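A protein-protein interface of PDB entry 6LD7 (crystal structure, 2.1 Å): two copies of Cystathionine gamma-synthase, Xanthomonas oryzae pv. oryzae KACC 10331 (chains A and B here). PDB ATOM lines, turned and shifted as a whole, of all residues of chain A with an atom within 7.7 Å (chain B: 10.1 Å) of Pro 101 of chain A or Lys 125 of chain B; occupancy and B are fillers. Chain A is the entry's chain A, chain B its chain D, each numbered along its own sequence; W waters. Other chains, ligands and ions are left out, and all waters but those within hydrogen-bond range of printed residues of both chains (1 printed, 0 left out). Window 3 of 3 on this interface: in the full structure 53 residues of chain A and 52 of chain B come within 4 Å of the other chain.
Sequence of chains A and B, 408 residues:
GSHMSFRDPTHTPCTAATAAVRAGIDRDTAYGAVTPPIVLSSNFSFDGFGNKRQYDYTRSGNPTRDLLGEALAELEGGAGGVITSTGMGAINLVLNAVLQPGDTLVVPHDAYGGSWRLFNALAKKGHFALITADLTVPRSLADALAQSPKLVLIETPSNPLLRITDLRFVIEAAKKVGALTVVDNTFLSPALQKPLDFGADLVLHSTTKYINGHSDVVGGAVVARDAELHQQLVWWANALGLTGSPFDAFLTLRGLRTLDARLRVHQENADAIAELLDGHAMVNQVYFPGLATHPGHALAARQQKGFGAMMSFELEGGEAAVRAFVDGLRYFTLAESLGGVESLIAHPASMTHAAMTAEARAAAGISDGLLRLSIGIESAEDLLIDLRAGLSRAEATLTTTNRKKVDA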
ATOM      1  N   LEU A  93      15.964 -22.590 -10.166  1.00  0.00           N
ATOM      2  CA  LEU A  93      15.541 -23.985 -10.070  1.00  0.00           C
ATOM      3  C   LEU A  93      14.630 -24.136  -8.847  1.00  0.00           C
ATOM      4  O   LEU A  93      13.605 -24.784  -8.972  1.00  0.00           O
ATOM      5  CB  LEU A  93      16.758 -24.903  -9.950  1.00  0.00           C
ATOM      6  CG  LEU A  93      16.451 -26.358  -9.634  1.00  0.00           C
ATOM      7  CD1 LEU A  93      15.574 -26.969 -10.704  1.00  0.00           C
ATOM      8  CD2 LEU A  93      17.747 -27.154  -9.516  1.00  0.00           C
ATOM      9  N   VAL A  94      15.066 -23.689  -7.673  1.00  0.00           N
ATOM     10  CA  VAL A  94      14.242 -23.784  -6.439  1.00  0.00           C
ATOM     11  C   VAL A  94      12.874 -23.096  -6.612  1.00  0.00           C
ATOM     12  O   VAL A  94      11.871 -23.745  -6.256  1.00  0.00           O
ATOM     13  CB  VAL A  94      15.013 -23.271  -5.199  1.00  0.00           C
ATOM     14  CG1 VAL A  94      14.096 -23.218  -3.984  1.00  0.00           C
ATOM     15  CG2 VAL A  94      16.200 -24.211  -4.933  1.00  0.00           C
ATOM     16  N   LEU A  95      12.808 -21.900  -7.194  1.00  0.00           N
ATOM     17  CA  LEU A  95      11.511 -21.188  -7.359  1.00  0.00           C
ATOM     18  C   LEU A  95      10.521 -22.010  -8.172  1.00  0.00           C
ATOM     19  O   LEU A  95       9.365 -22.097  -7.762  1.00  0.00           O
ATOM     20  CB  LEU A  95      11.754 -19.833  -8.007  1.00  0.00           C
ATOM     21  CG  LEU A  95      12.640 -18.893  -7.200  1.00  0.00           C
ATOM     22  CD1 LEU A  95      12.855 -17.622  -7.988  1.00  0.00           C
ATOM     23  CD2 LEU A  95      12.046 -18.601  -5.841  1.00  0.00           C
ATOM     24  N   ASN A  96      11.002 -22.656  -9.253  1.00  0.00           N
ATOM     25  CA  ASN A  96      10.202 -23.449 -10.211  1.00  0.00           C
ATOM     26  C   ASN A  96       9.866 -24.774  -9.561  1.00  0.00           C
ATOM     27  O   ASN A  96       8.734 -25.186  -9.712  1.00  0.00           O
ATOM     28  CB  ASN A  96      10.934 -23.685 -11.556  1.00  0.00           C
ATOM     29  CG  ASN A  96      10.817 -22.489 -12.449  1.00  0.00           C
ATOM     30  OD1 ASN A  96       9.823 -22.379 -13.186  1.00  0.00           O
ATOM     31  ND2 ASN A  96      11.751 -21.550 -12.326  1.00  0.00           N
ATOM     32  N   ALA A  97      10.768 -25.397  -8.798  1.00  0.00           N
ATOM     33  CA  ALA A  97      10.458 -26.699  -8.219  1.00  0.00           C
ATOM     34  C   ALA A  97       9.420 -26.498  -7.100  1.00  0.00           C
ATOM     35  O   ALA A  97       8.718 -27.384  -6.817  1.00  0.00           O
ATOM     36  CB  ALA A  97      11.671 -27.344  -7.635  1.00  0.00           C
ATOM     37  N   VAL A  98       9.434 -25.387  -6.390  1.00  0.00           N
ATOM     38  CA  VAL A  98       8.757 -25.332  -5.058  1.00  0.00           C
ATOM     39  C   VAL A  98       7.475 -24.519  -5.184  1.00  0.00           C
ATOM     40  O   VAL A  98       6.572 -24.910  -4.508  1.00  0.00           O
ATOM     41  CB  VAL A  98       9.660 -24.800  -3.923  1.00  0.00           C
ATOM     42  CG1 VAL A  98       8.877 -24.582  -2.640  1.00  0.00           C
ATOM     43  CG2 VAL A  98      10.775 -25.777  -3.661  1.00  0.00           C
ATOM     44  N   LEU A  99       7.451 -23.424  -5.950  1.00  0.00           N
ATOM     45  CA  LEU A  99       6.333 -22.472  -5.918  1.00  0.00           C
ATOM     46  C   LEU A  99       5.411 -22.595  -7.136  1.00  0.00           C
ATOM     47  O   LEU A  99       5.860 -22.904  -8.272  1.00  0.00           O
ATOM     48  CB  LEU A  99       6.917 -21.074  -5.886  1.00  0.00           C
ATOM     49  CG  LEU A  99       7.824 -20.742  -4.707  1.00  0.00           C
ATOM     50  CD1 LEU A  99       8.496 -19.368  -4.912  1.00  0.00           C
ATOM     51  CD2 LEU A  99       7.013 -20.769  -3.434  1.00  0.00           C
ATOM     52  N   GLN A 100       4.181 -22.193  -6.931  1.00  0.00           N
ATOM     53  CA  GLN A 100       3.182 -21.985  -8.000  1.00  0.00           C
ATOM     54  C   GLN A 100       2.301 -20.793  -7.637  1.00  0.00           C
ATOM     55  O   GLN A 100       2.314 -20.326  -6.490  1.00  0.00           O
ATOM     56  CB  GLN A 100       2.391 -23.268  -8.183  1.00  0.00           C
ATOM     57  CG  GLN A 100       1.465 -23.591  -7.032  1.00  0.00           C
ATOM     58  CD  GLN A 100       0.694 -24.823  -7.431  1.00  0.00           C
ATOM     59  OE1 GLN A 100       0.137 -25.513  -6.618  1.00  0.00           O
ATOM     60  NE2 GLN A 100       0.704 -25.149  -8.712  1.00  0.00           N
ATOM     61  N   PRO A 101       1.585 -20.235  -8.630  1.00  0.00           N
ATOM     62  CA  PRO A 101       0.838 -18.990  -8.452  1.00  0.00           C
ATOM     63  C   PRO A 101      -0.096 -19.187  -7.255  1.00  0.00           C
ATOM     64  O   PRO A 101      -0.524 -20.304  -6.974  1.00  0.00           O
ATOM     65  CB  PRO A 101       0.125 -18.756  -9.805  1.00  0.00           C
ATOM     66  CG  PRO A 101       1.006 -19.492 -10.777  1.00  0.00           C
ATOM     67  CD  PRO A 101       1.534 -20.712 -10.028  1.00  0.00           C
ATOM     68  N   GLY A 102      -0.250 -18.165  -6.431  1.00  0.00           N
ATOM     69  CA  GLY A 102      -1.028 -18.366  -5.203  1.00  0.00           C
ATOM     70  C   GLY A 102      -0.119 -18.585  -4.020  1.00  0.00           C
ATOM     71  O   GLY A 102      -0.593 -18.388  -2.928  1.00  0.00           O
ATOM     72  N   ASP A 103       1.090 -19.125  -4.217  1.00  0.00           N
ATOM     73  CA  ASP A 103       2.016 -19.382  -3.093  1.00  0.00           C
ATOM     74  C   ASP A 103       2.702 -18.060  -2.756  1.00  0.00           C
ATOM     75  O   ASP A 103       2.869 -17.169  -3.671  1.00  0.00           O
ATOM     76  CB  ASP A 103       3.055 -20.459  -3.336  1.00  0.00           C
ATOM     77  CG  ASP A 103       2.604 -21.890  -3.559  1.00  0.00           C
ATOM     78  OD1 ASP A 103       1.575 -22.245  -3.083  1.00  0.00           O
ATOM     79  OD2 ASP A 103       3.332 -22.650  -4.250  1.00  0.00           O
ATOM     80  N   THR A 104       3.164 -17.952  -1.504  1.00  0.00           N
ATOM     81  CA  THR A 104       4.008 -16.799  -1.157  1.00  0.00           C
ATOM     82  C   THR A 104       5.407 -17.274  -0.727  1.00  0.00           C
ATOM     83  O   THR A 104       5.593 -18.362  -0.142  1.00  0.00           O
ATOM     84  CB  THR A 104       3.195 -15.738  -0.348  1.00  0.00           C
ATOM     85  OG1 THR A 104       3.877 -15.314   0.819  1.00  0.00           O
ATOM     86  CG2 THR A 104       1.782 -16.100  -0.014  1.00  0.00           C
ATOM     87  N   LYS A 125       5.081 -10.785 -12.557  1.00  0.00           N
ATOM     88  CA  LYS A 125       4.253 -11.549 -13.511  1.00  0.00           C
ATOM     89  C   LYS A 125       3.247 -12.454 -12.810  1.00  0.00           C
ATOM     90  O   LYS A 125       2.469 -13.045 -13.494  1.00  0.00           O
ATOM     91  CB  LYS A 125       5.094 -12.507 -14.327  1.00  0.00           C
ATOM     92  CG  LYS A 125       6.013 -11.873 -15.338  1.00  0.00           C
ATOM     93  CD  LYS A 125       6.751 -12.950 -16.047  1.00  0.00           C
ATOM     94  CE  LYS A 125       7.156 -12.669 -17.480  1.00  0.00           C
ATOM     95  NZ  LYS A 125       7.888 -13.896 -17.838  1.00  0.00           N
ATOM     96  N   GLY A 126       3.265 -12.609 -11.504  1.00  0.00           N
ATOM     97  CA  GLY A 126       2.263 -13.425 -10.798  1.00  0.00           C
ATOM     98  C   GLY A 126       2.671 -14.883 -10.668  1.00  0.00           C
ATOM     99  O   GLY A 126       1.803 -15.731 -10.353  1.00  0.00           O
ATOM    100  N   HIS A 127       3.957 -15.218 -10.724  1.00  0.00           N
ATOM    101  CA  HIS A 127       4.338 -16.634 -10.517  1.00  0.00           C
ATOM    102  C   HIS A 127       4.113 -17.015  -9.051  1.00  0.00           C
ATOM    103  O   HIS A 127       4.028 -18.242  -8.754  1.00  0.00           O
ATOM    104  CB  HIS A 127       5.783 -16.875 -11.018  1.00  0.00           C
ATOM    105  CG  HIS A 127       5.932 -16.800 -12.496  1.00  0.00           C
ATOM    106  ND1 HIS A 127       7.046 -17.330 -13.154  1.00  0.00           N
ATOM    107  CD2 HIS A 127       5.091 -16.337 -13.461  1.00  0.00           C
ATOM    108  CE1 HIS A 127       6.875 -17.174 -14.459  1.00  0.00           C
ATOM    109  NE2 HIS A 127       5.707 -16.547 -14.665  1.00  0.00           N
ATOM    110  N   PHE A 128       4.217 -16.035  -8.150  1.00  0.00           N
ATOM    111  CA  PHE A 128       4.012 -16.173  -6.675  1.00  0.00           C
ATOM    112  C   PHE A 128       3.897 -14.779  -6.065  1.00  0.00           C
ATOM    113  O   PHE A 128       4.133 -13.794  -6.738  1.00  0.00           O
ATOM    114  CB  PHE A 128       5.163 -16.938  -5.999  1.00  0.00           C
ATOM    115  CG  PHE A 128       6.530 -16.511  -6.433  1.00  0.00           C
ATOM    116  CD1 PHE A 128       7.140 -15.388  -5.898  1.00  0.00           C
ATOM    117  CD2 PHE A 128       7.161 -17.179  -7.472  1.00  0.00           C
ATOM    118  CE1 PHE A 128       8.399 -14.990  -6.348  1.00  0.00           C
ATOM    119  CE2 PHE A 128       8.401 -16.781  -7.920  1.00  0.00           C
ATOM    120  CZ  PHE A 128       9.030 -15.703  -7.343  1.00  0.00           C
ATOM    121  N   ALA A 129       3.530 -14.667  -4.805  1.00  0.00           N
ATOM    122  CA  ALA A 129       3.160 -13.346  -4.252  1.00  0.00           C
ATOM    123  C   ALA A 129       4.375 -12.564  -3.726  1.00  0.00           C
ATOM    124  O   ALA A 129       4.349 -11.288  -3.973  1.00  0.00           O
ATOM    125  CB  ALA A 129       2.083 -13.464  -3.177  1.00  0.00           C
ATOM    126  N   TRP A 236      13.176 -30.979 -12.516  1.00  0.00           N
ATOM    127  CA  TRP A 236      12.964 -29.599 -13.007  1.00  0.00           C
ATOM    128  C   TRP A 236      14.214 -29.108 -13.710  1.00  0.00           C
ATOM    129  O   TRP A 236      14.113 -28.318 -14.646  1.00  0.00           O
ATOM    130  CB  TRP A 236      12.542 -28.664 -11.872  1.00  0.00           C
ATOM    131  CG  TRP A 236      11.081 -28.724 -11.583  1.00  0.00           C
ATOM    132  CD1 TRP A 236      10.485 -29.476 -10.601  1.00  0.00           C
ATOM    133  CD2 TRP A 236      10.023 -28.098 -12.337  1.00  0.00           C
ATOM    134  NE1 TRP A 236       9.140 -29.301 -10.682  1.00  0.00           N
ATOM    135  CE2 TRP A 236       8.816 -28.488 -11.730  1.00  0.00           C
ATOM    136  CE3 TRP A 236       9.977 -27.244 -13.446  1.00  0.00           C
ATOM    137  CZ2 TRP A 236       7.561 -28.054 -12.181  1.00  0.00           C
ATOM    138  CZ3 TRP A 236       8.737 -26.852 -13.938  1.00  0.00           C
ATOM    139  CH2 TRP A 236       7.549 -27.205 -13.266  1.00  0.00           C
ATOM    140  N   LEU A 240      13.769 -27.619 -17.352  1.00  0.00           N
ATOM    141  CA  LEU A 240      14.056 -26.190 -17.604  1.00  0.00           C
ATOM    142  C   LEU A 240      15.403 -26.016 -18.341  1.00  0.00           C
ATOM    143  O   LEU A 240      15.715 -24.915 -18.782  1.00  0.00           O
ATOM    144  CB  LEU A 240      14.113 -25.463 -16.258  1.00  0.00           C
ATOM    145  CG  LEU A 240      12.811 -25.401 -15.461  1.00  0.00           C
ATOM    146  CD1 LEU A 240      13.014 -24.935 -14.019  1.00  0.00           C
ATOM    147  CD2 LEU A 240      11.877 -24.438 -16.107  1.00  0.00           C
ATOM    148  N   GLN B 100       3.477 -14.026 -20.216  1.00  0.00           N
ATOM    149  CA  GLN B 100       3.019 -13.807 -18.828  1.00  0.00           C
ATOM    150  C   GLN B 100       1.599 -14.358 -18.690  1.00  0.00           C
ATOM    151  O   GLN B 100       0.945 -14.688 -19.694  1.00  0.00           O
ATOM    152  CB  GLN B 100       3.130 -12.318 -18.490  1.00  0.00           C
ATOM    153  CG  GLN B 100       2.104 -11.473 -19.199  1.00  0.00           C
ATOM    154  CD  GLN B 100       2.244 -10.042 -18.743  1.00  0.00           C
ATOM    155  OE1 GLN B 100       1.399  -9.228 -19.006  1.00  0.00           O
ATOM    156  NE2 GLN B 100       3.269  -9.735 -17.974  1.00  0.00           N
ATOM    157  N   PRO B 101       1.123 -14.547 -17.443  1.00  0.00           N
ATOM    158  CA  PRO B 101      -0.142 -15.240 -17.190  1.00  0.00           C
ATOM    159  C   PRO B 101      -1.219 -14.455 -17.956  1.00  0.00           C
ATOM    160  O   PRO B 101      -1.090 -13.231 -18.170  1.00  0.00           O
ATOM    161  CB  PRO B 101      -0.287 -15.293 -15.643  1.00  0.00           C
ATOM    162  CG  PRO B 101       1.136 -15.143 -15.179  1.00  0.00           C
ATOM    163  CD  PRO B 101       1.822 -14.211 -16.182  1.00  0.00           C
ATOM    164  N   GLY B 102      -2.155 -15.181 -18.553  1.00  0.00           N
ATOM    165  CA  GLY B 102      -3.143 -14.527 -19.414  1.00  0.00           C
ATOM    166  C   GLY B 102      -2.761 -14.625 -20.874  1.00  0.00           C
ATOM    167  O   GLY B 102      -3.625 -14.389 -21.711  1.00  0.00           O
ATOM    168  N   ARG B 117       7.130 -31.257 -22.675  1.00  0.00           N
ATOM    169  CA  ARG B 117       7.225 -31.489 -21.205  1.00  0.00           C
ATOM    170  C   ARG B 117       7.279 -30.118 -20.494  1.00  0.00           C
ATOM    171  O   ARG B 117       6.590 -29.903 -19.468  1.00  0.00           O
ATOM    172  CB  ARG B 117       8.419 -32.411 -20.939  1.00  0.00           C
ATOM    173  CG  ARG B 117       8.652 -32.785 -19.481  1.00  0.00           C
ATOM    174  CD  ARG B 117      10.087 -33.000 -19.078  1.00  0.00           C
ATOM    175  NE  ARG B 117      10.865 -33.991 -19.791  1.00  0.00           N
ATOM    176  CZ  ARG B 117      12.032 -33.791 -20.468  1.00  0.00           C
ATOM    177  NH1 ARG B 117      12.578 -34.829 -21.072  1.00  0.00           N
ATOM    178  NH2 ARG B 117      12.651 -32.616 -20.618  1.00  0.00           N
ATOM    179  N   LEU B 118       8.062 -29.195 -21.030  1.00  0.00           N
ATOM    180  CA  LEU B 118       8.229 -27.861 -20.435  1.00  0.00           C
ATOM    181  C   LEU B 118       6.930 -27.108 -20.632  1.00  0.00           C
ATOM    182  O   LEU B 118       6.509 -26.453 -19.672  1.00  0.00           O
ATOM    183  CB  LEU B 118       9.387 -27.098 -21.094  1.00  0.00           C
ATOM    184  CG  LEU B 118       9.687 -25.733 -20.518  1.00  0.00           C
ATOM    185  CD1 LEU B 118       9.884 -25.823 -19.009  1.00  0.00           C
ATOM    186  CD2 LEU B 118      10.881 -25.102 -21.202  1.00  0.00           C
ATOM    187  N   PHE B 119       6.366 -27.112 -21.853  1.00  0.00           N
ATOM    188  CA  PHE B 119       5.122 -26.336 -22.097  1.00  0.00           C
ATOM    189  C   PHE B 119       4.058 -26.808 -21.124  1.00  0.00           C
ATOM    190  O   PHE B 119       3.403 -26.007 -20.544  1.00  0.00           O
ATOM    191  CB  PHE B 119       4.629 -26.454 -23.531  1.00  0.00           C
ATOM    192  CG  PHE B 119       5.584 -25.962 -24.579  1.00  0.00           C
ATOM    193  CD1 PHE B 119       6.522 -24.999 -24.301  1.00  0.00           C
ATOM    194  CD2 PHE B 119       5.610 -26.548 -25.824  1.00  0.00           C
ATOM    195  CE1 PHE B 119       7.404 -24.566 -25.279  1.00  0.00           C
ATOM    196  CE2 PHE B 119       6.523 -26.147 -26.785  1.00  0.00           C
ATOM    197  CZ  PHE B 119       7.386 -25.125 -26.517  1.00  0.00           C
ATOM    198  N   ASN B 120       3.909 -28.106 -20.964  1.00  0.00           N
ATOM    199  CA  ASN B 120       2.832 -28.665 -20.127  1.00  0.00           C
ATOM    200  C   ASN B 120       3.032 -28.282 -18.654  1.00  0.00           C
ATOM    201  O   ASN B 120       2.061 -27.913 -18.009  1.00  0.00           O
ATOM    202  CB  ASN B 120       2.845 -30.179 -20.284  1.00  0.00           C
ATOM    203  CG  ASN B 120       1.497 -30.583 -20.785  1.00  0.00           C
ATOM    204  OD1 ASN B 120       1.141 -30.252 -21.942  1.00  0.00           O
ATOM    205  ND2 ASN B 120       0.727 -31.096 -19.829  1.00  0.00           N
ATOM    206  N   ALA B 121       4.245 -28.454 -18.114  1.00  0.00           N
ATOM    207  CA  ALA B 121       4.566 -28.132 -16.707  1.00  0.00           C
ATOM    208  C   ALA B 121       4.264 -26.659 -16.421  1.00  0.00           C
ATOM    209  O   ALA B 121       3.627 -26.357 -15.373  1.00  0.00           O
ATOM    210  CB  ALA B 121       6.015 -28.435 -16.439  1.00  0.00           C
ATOM    211  N   LEU B 122       4.744 -25.747 -17.257  1.00  0.00           N
ATOM    212  CA  LEU B 122       4.511 -24.305 -17.015  1.00  0.00           C
ATOM    213  C   LEU B 122       3.034 -23.921 -17.243  1.00  0.00           C
ATOM    214  O   LEU B 122       2.522 -23.109 -16.435  1.00  0.00           O
ATOM    215  CB  LEU B 122       5.463 -23.498 -17.869  1.00  0.00           C
ATOM    216  CG  LEU B 122       6.937 -23.733 -17.566  1.00  0.00           C
ATOM    217  CD1 LEU B 122       7.820 -22.932 -18.513  1.00  0.00           C
ATOM    218  CD2 LEU B 122       7.260 -23.401 -16.096  1.00  0.00           C
ATOM    219  N   ALA B 123       2.330 -24.538 -18.203  1.00  0.00           N
ATOM    220  CA  ALA B 123       0.901 -24.221 -18.415  1.00  0.00           C
ATOM    221  C   ALA B 123       0.107 -24.732 -17.222  1.00  0.00           C
ATOM    222  O   ALA B 123      -0.780 -24.033 -16.879  1.00  0.00           O
ATOM    223  CB  ALA B 123       0.313 -24.832 -19.686  1.00  0.00           C
ATOM    224  N   LYS B 124       0.380 -25.938 -16.723  1.00  0.00           N
ATOM    225  CA  LYS B 124      -0.304 -26.575 -15.586  1.00  0.00           C
ATOM    226  C   LYS B 124      -0.182 -25.675 -14.353  1.00  0.00           C
ATOM    227  O   LYS B 124      -1.032 -25.734 -13.561  1.00  0.00           O
ATOM    228  CB  LYS B 124       0.331 -27.917 -15.241  1.00  0.00           C
ATOM    229  CG  LYS B 124      -0.599 -29.108 -15.317  1.00  0.00           C
ATOM    230  CD  LYS B 124       0.064 -30.401 -15.802  1.00  0.00           C
ATOM    231  CE  LYS B 124       0.687 -31.217 -14.682  1.00  0.00           C
ATOM    232  NZ  LYS B 124       1.755 -32.104 -15.220  1.00  0.00           N
ATOM    233  N   LYS B 125       0.885 -24.903 -14.196  1.00  0.00           N
ATOM    234  CA  LYS B 125       0.981 -23.877 -13.135  1.00  0.00           C
ATOM    235  C   LYS B 125       0.395 -22.518 -13.549  1.00  0.00           C
ATOM    236  O   LYS B 125       0.421 -21.639 -12.750  1.00  0.00           O
ATOM    237  CB  LYS B 125       2.428 -23.550 -12.826  1.00  0.00           C
ATOM    238  CG  LYS B 125       3.252 -24.675 -12.264  1.00  0.00           C
ATOM    239  CD  LYS B 125       4.626 -24.170 -11.903  1.00  0.00           C
ATOM    240  CE  LYS B 125       5.244 -24.946 -10.762  1.00  0.00           C
ATOM    241  NZ  LYS B 125       6.553 -24.337 -10.573  1.00  0.00           N
ATOM    242  N   GLY B 126      -0.116 -22.315 -14.747  1.00  0.00           N
ATOM    243  CA  GLY B 126      -0.720 -21.022 -15.124  1.00  0.00           C
ATOM    244  C   GLY B 126       0.311 -19.973 -15.500  1.00  0.00           C
ATOM    245  O   GLY B 126      -0.044 -18.807 -15.488  1.00  0.00           O
ATOM    246  N   HIS B 127       1.515 -20.301 -15.993  1.00  0.00           N
ATOM    247  CA  HIS B 127       2.411 -19.224 -16.476  1.00  0.00           C
ATOM    248  C   HIS B 127       1.812 -18.619 -17.746  1.00  0.00           C
ATOM    249  O   HIS B 127       2.160 -17.462 -18.127  1.00  0.00           O
ATOM    250  CB  HIS B 127       3.863 -19.731 -16.616  1.00  0.00           C
ATOM    251  CG  HIS B 127       4.566 -20.051 -15.342  1.00  0.00           C
ATOM    252  ND1 HIS B 127       3.935 -20.048 -14.098  1.00  0.00           N
ATOM    253  CD2 HIS B 127       5.874 -20.275 -15.078  1.00  0.00           C
ATOM    254  CE1 HIS B 127       4.818 -20.325 -13.158  1.00  0.00           C
ATOM    255  NE2 HIS B 127       6.004 -20.459 -13.725  1.00  0.00           N
ATOM    256  N   PHE B 128       1.031 -19.420 -18.470  1.00  0.00           N
ATOM    257  CA  PHE B 128       0.372 -19.039 -19.754  1.00  0.00           C
ATOM    258  C   PHE B 128      -0.607 -20.149 -20.120  1.00  0.00           C
ATOM    259  O   PHE B 128      -0.596 -21.231 -19.528  1.00  0.00           O
ATOM    260  CB  PHE B 128       1.369 -18.848 -20.919  1.00  0.00           C
ATOM    261  CG  PHE B 128       2.420 -19.916 -21.010  1.00  0.00           C
ATOM    262  CD1 PHE B 128       2.179 -21.107 -21.657  1.00  0.00           C
ATOM    263  CD2 PHE B 128       3.656 -19.744 -20.396  1.00  0.00           C
ATOM    264  CE1 PHE B 128       3.145 -22.109 -21.696  1.00  0.00           C
ATOM    265  CE2 PHE B 128       4.620 -20.733 -20.446  1.00  0.00           C
ATOM    266  CZ  PHE B 128       4.369 -21.922 -21.077  1.00  0.00           C
ATOM    267  N   ALA B 129      -1.470 -19.893 -21.081  1.00  0.00           N
ATOM    268  CA  ALA B 129      -2.386 -20.930 -21.604  1.00  0.00           C
ATOM    269  C   ALA B 129      -1.725 -21.476 -22.900  1.00  0.00           C
ATOM    270  O   ALA B 129      -1.083 -20.692 -23.675  1.00  0.00           O
ATOM    271  CB  ALA B 129      -3.777 -20.311 -21.852  1.00  0.00           C
ATOM    272  N   LEU B 130      -1.910 -22.762 -23.134  1.00  0.00           N
ATOM    273  CA  LEU B 130      -1.337 -23.534 -24.231  1.00  0.00           C
ATOM    274  C   LEU B 130      -2.443 -23.814 -25.241  1.00  0.00           C
ATOM    275  O   LEU B 130      -3.436 -24.336 -24.817  1.00  0.00           O
ATOM    276  CB  LEU B 130      -0.934 -24.875 -23.620  1.00  0.00           C
ATOM    277  CG  LEU B 130       0.500 -25.288 -23.759  1.00  0.00           C
ATOM    278  CD1 LEU B 130       0.616 -26.794 -23.557  1.00  0.00           C
ATOM    279  CD2 LEU B 130       1.071 -24.809 -25.081  1.00  0.00           C
HETATM  280  O   HOH W   1       4.482 -16.314 -17.176  1.00  0.00           O
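The backbone carbonyl oxygen of Asn 96 of chain A sits at hydrogen-bond distance from the side-chain amino group of Lys 125 of chain B.
O of Leu 99 of chain A sits at hydrogen-bond distance from NZ of Lys 125 of chain B (2.8 Å).
A ring nitrogen (NE2) of His 127 of chain B lies within hydrogen-bond range of a ring nitrogen (ND1) of His 127 of chain A (3.3 Å).
O of Leu 122 of chain B is in hydrogen-bond range of N of His 127 of chain B, at 3.0 Å.
Among the printed residues, merely in contact across the chains: Pro 101 of chain A with Lys 125 of chain B (3.0 Å), Lys 125 of chain A with Pro 101 of chain B (3.0 Å), Trp 236 of chain A with Ala 121 of chain B (3.7 Å) and Leu 240 of chain A with Leu 118 of chain B (3.8 Å).
Pro 101 of chain A touches just one residue of chain B: Lys 125.
Lys 125 of chain B touches three residues of chain A.
Gln 100 of chain A touches none of the printed residues of chain B.
No residue of chain B comes within 4 Å of Asp 103 of chain A.
Of the printed residues of chain B, His 127 of chain A touches His 127 (3.3 Å).
Printed residues of chain B within 4 Å of Leu 99 of chain A: Lys 125 (2.8 Å).
Printed residues of chain B within 4 Å of Trp 236 of chain A: Ala 121 (3.7 Å).
Arg 117 of chain B touches none of the printed residues of chain A.
The nearest residue of chain A that does not touch Lys 125 of chain B is Trp 236 of chain A (4.1 Å).
The nearest printed residue of chain B that does not touch Lys 125 of chain A is Gln 100 of chain B (4.2 Å).
Of the 17 printed residues of chain B, 5 touch a printed residue of chain A.
Of the 19 printed residues of chain A, 7 touch a printed residue of chain B.
Printed residues of chain A that touch a printed residue of chain B: Asn 96, Leu 99, Pro 101, Lys 125, His 127, Trp 236 and Leu 240.
Among the printed residues, no Asp or Glu carboxylate lies within 4 Å of a Lys or Arg side-chain nitrogen of the other chain.
Pro 101 of chain A touches Lys 125 of chain B, and with the chains exchanged Lys 125 of chain A touches Pro 101 of chain B.
His 127 of chain A touches its own counterpart, His 127 of chain B.
Water W1 bridges the backbone carbonyl oxygen of His 127 of chain B and a ring nitrogen (NE2) of His 127 of chain A.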
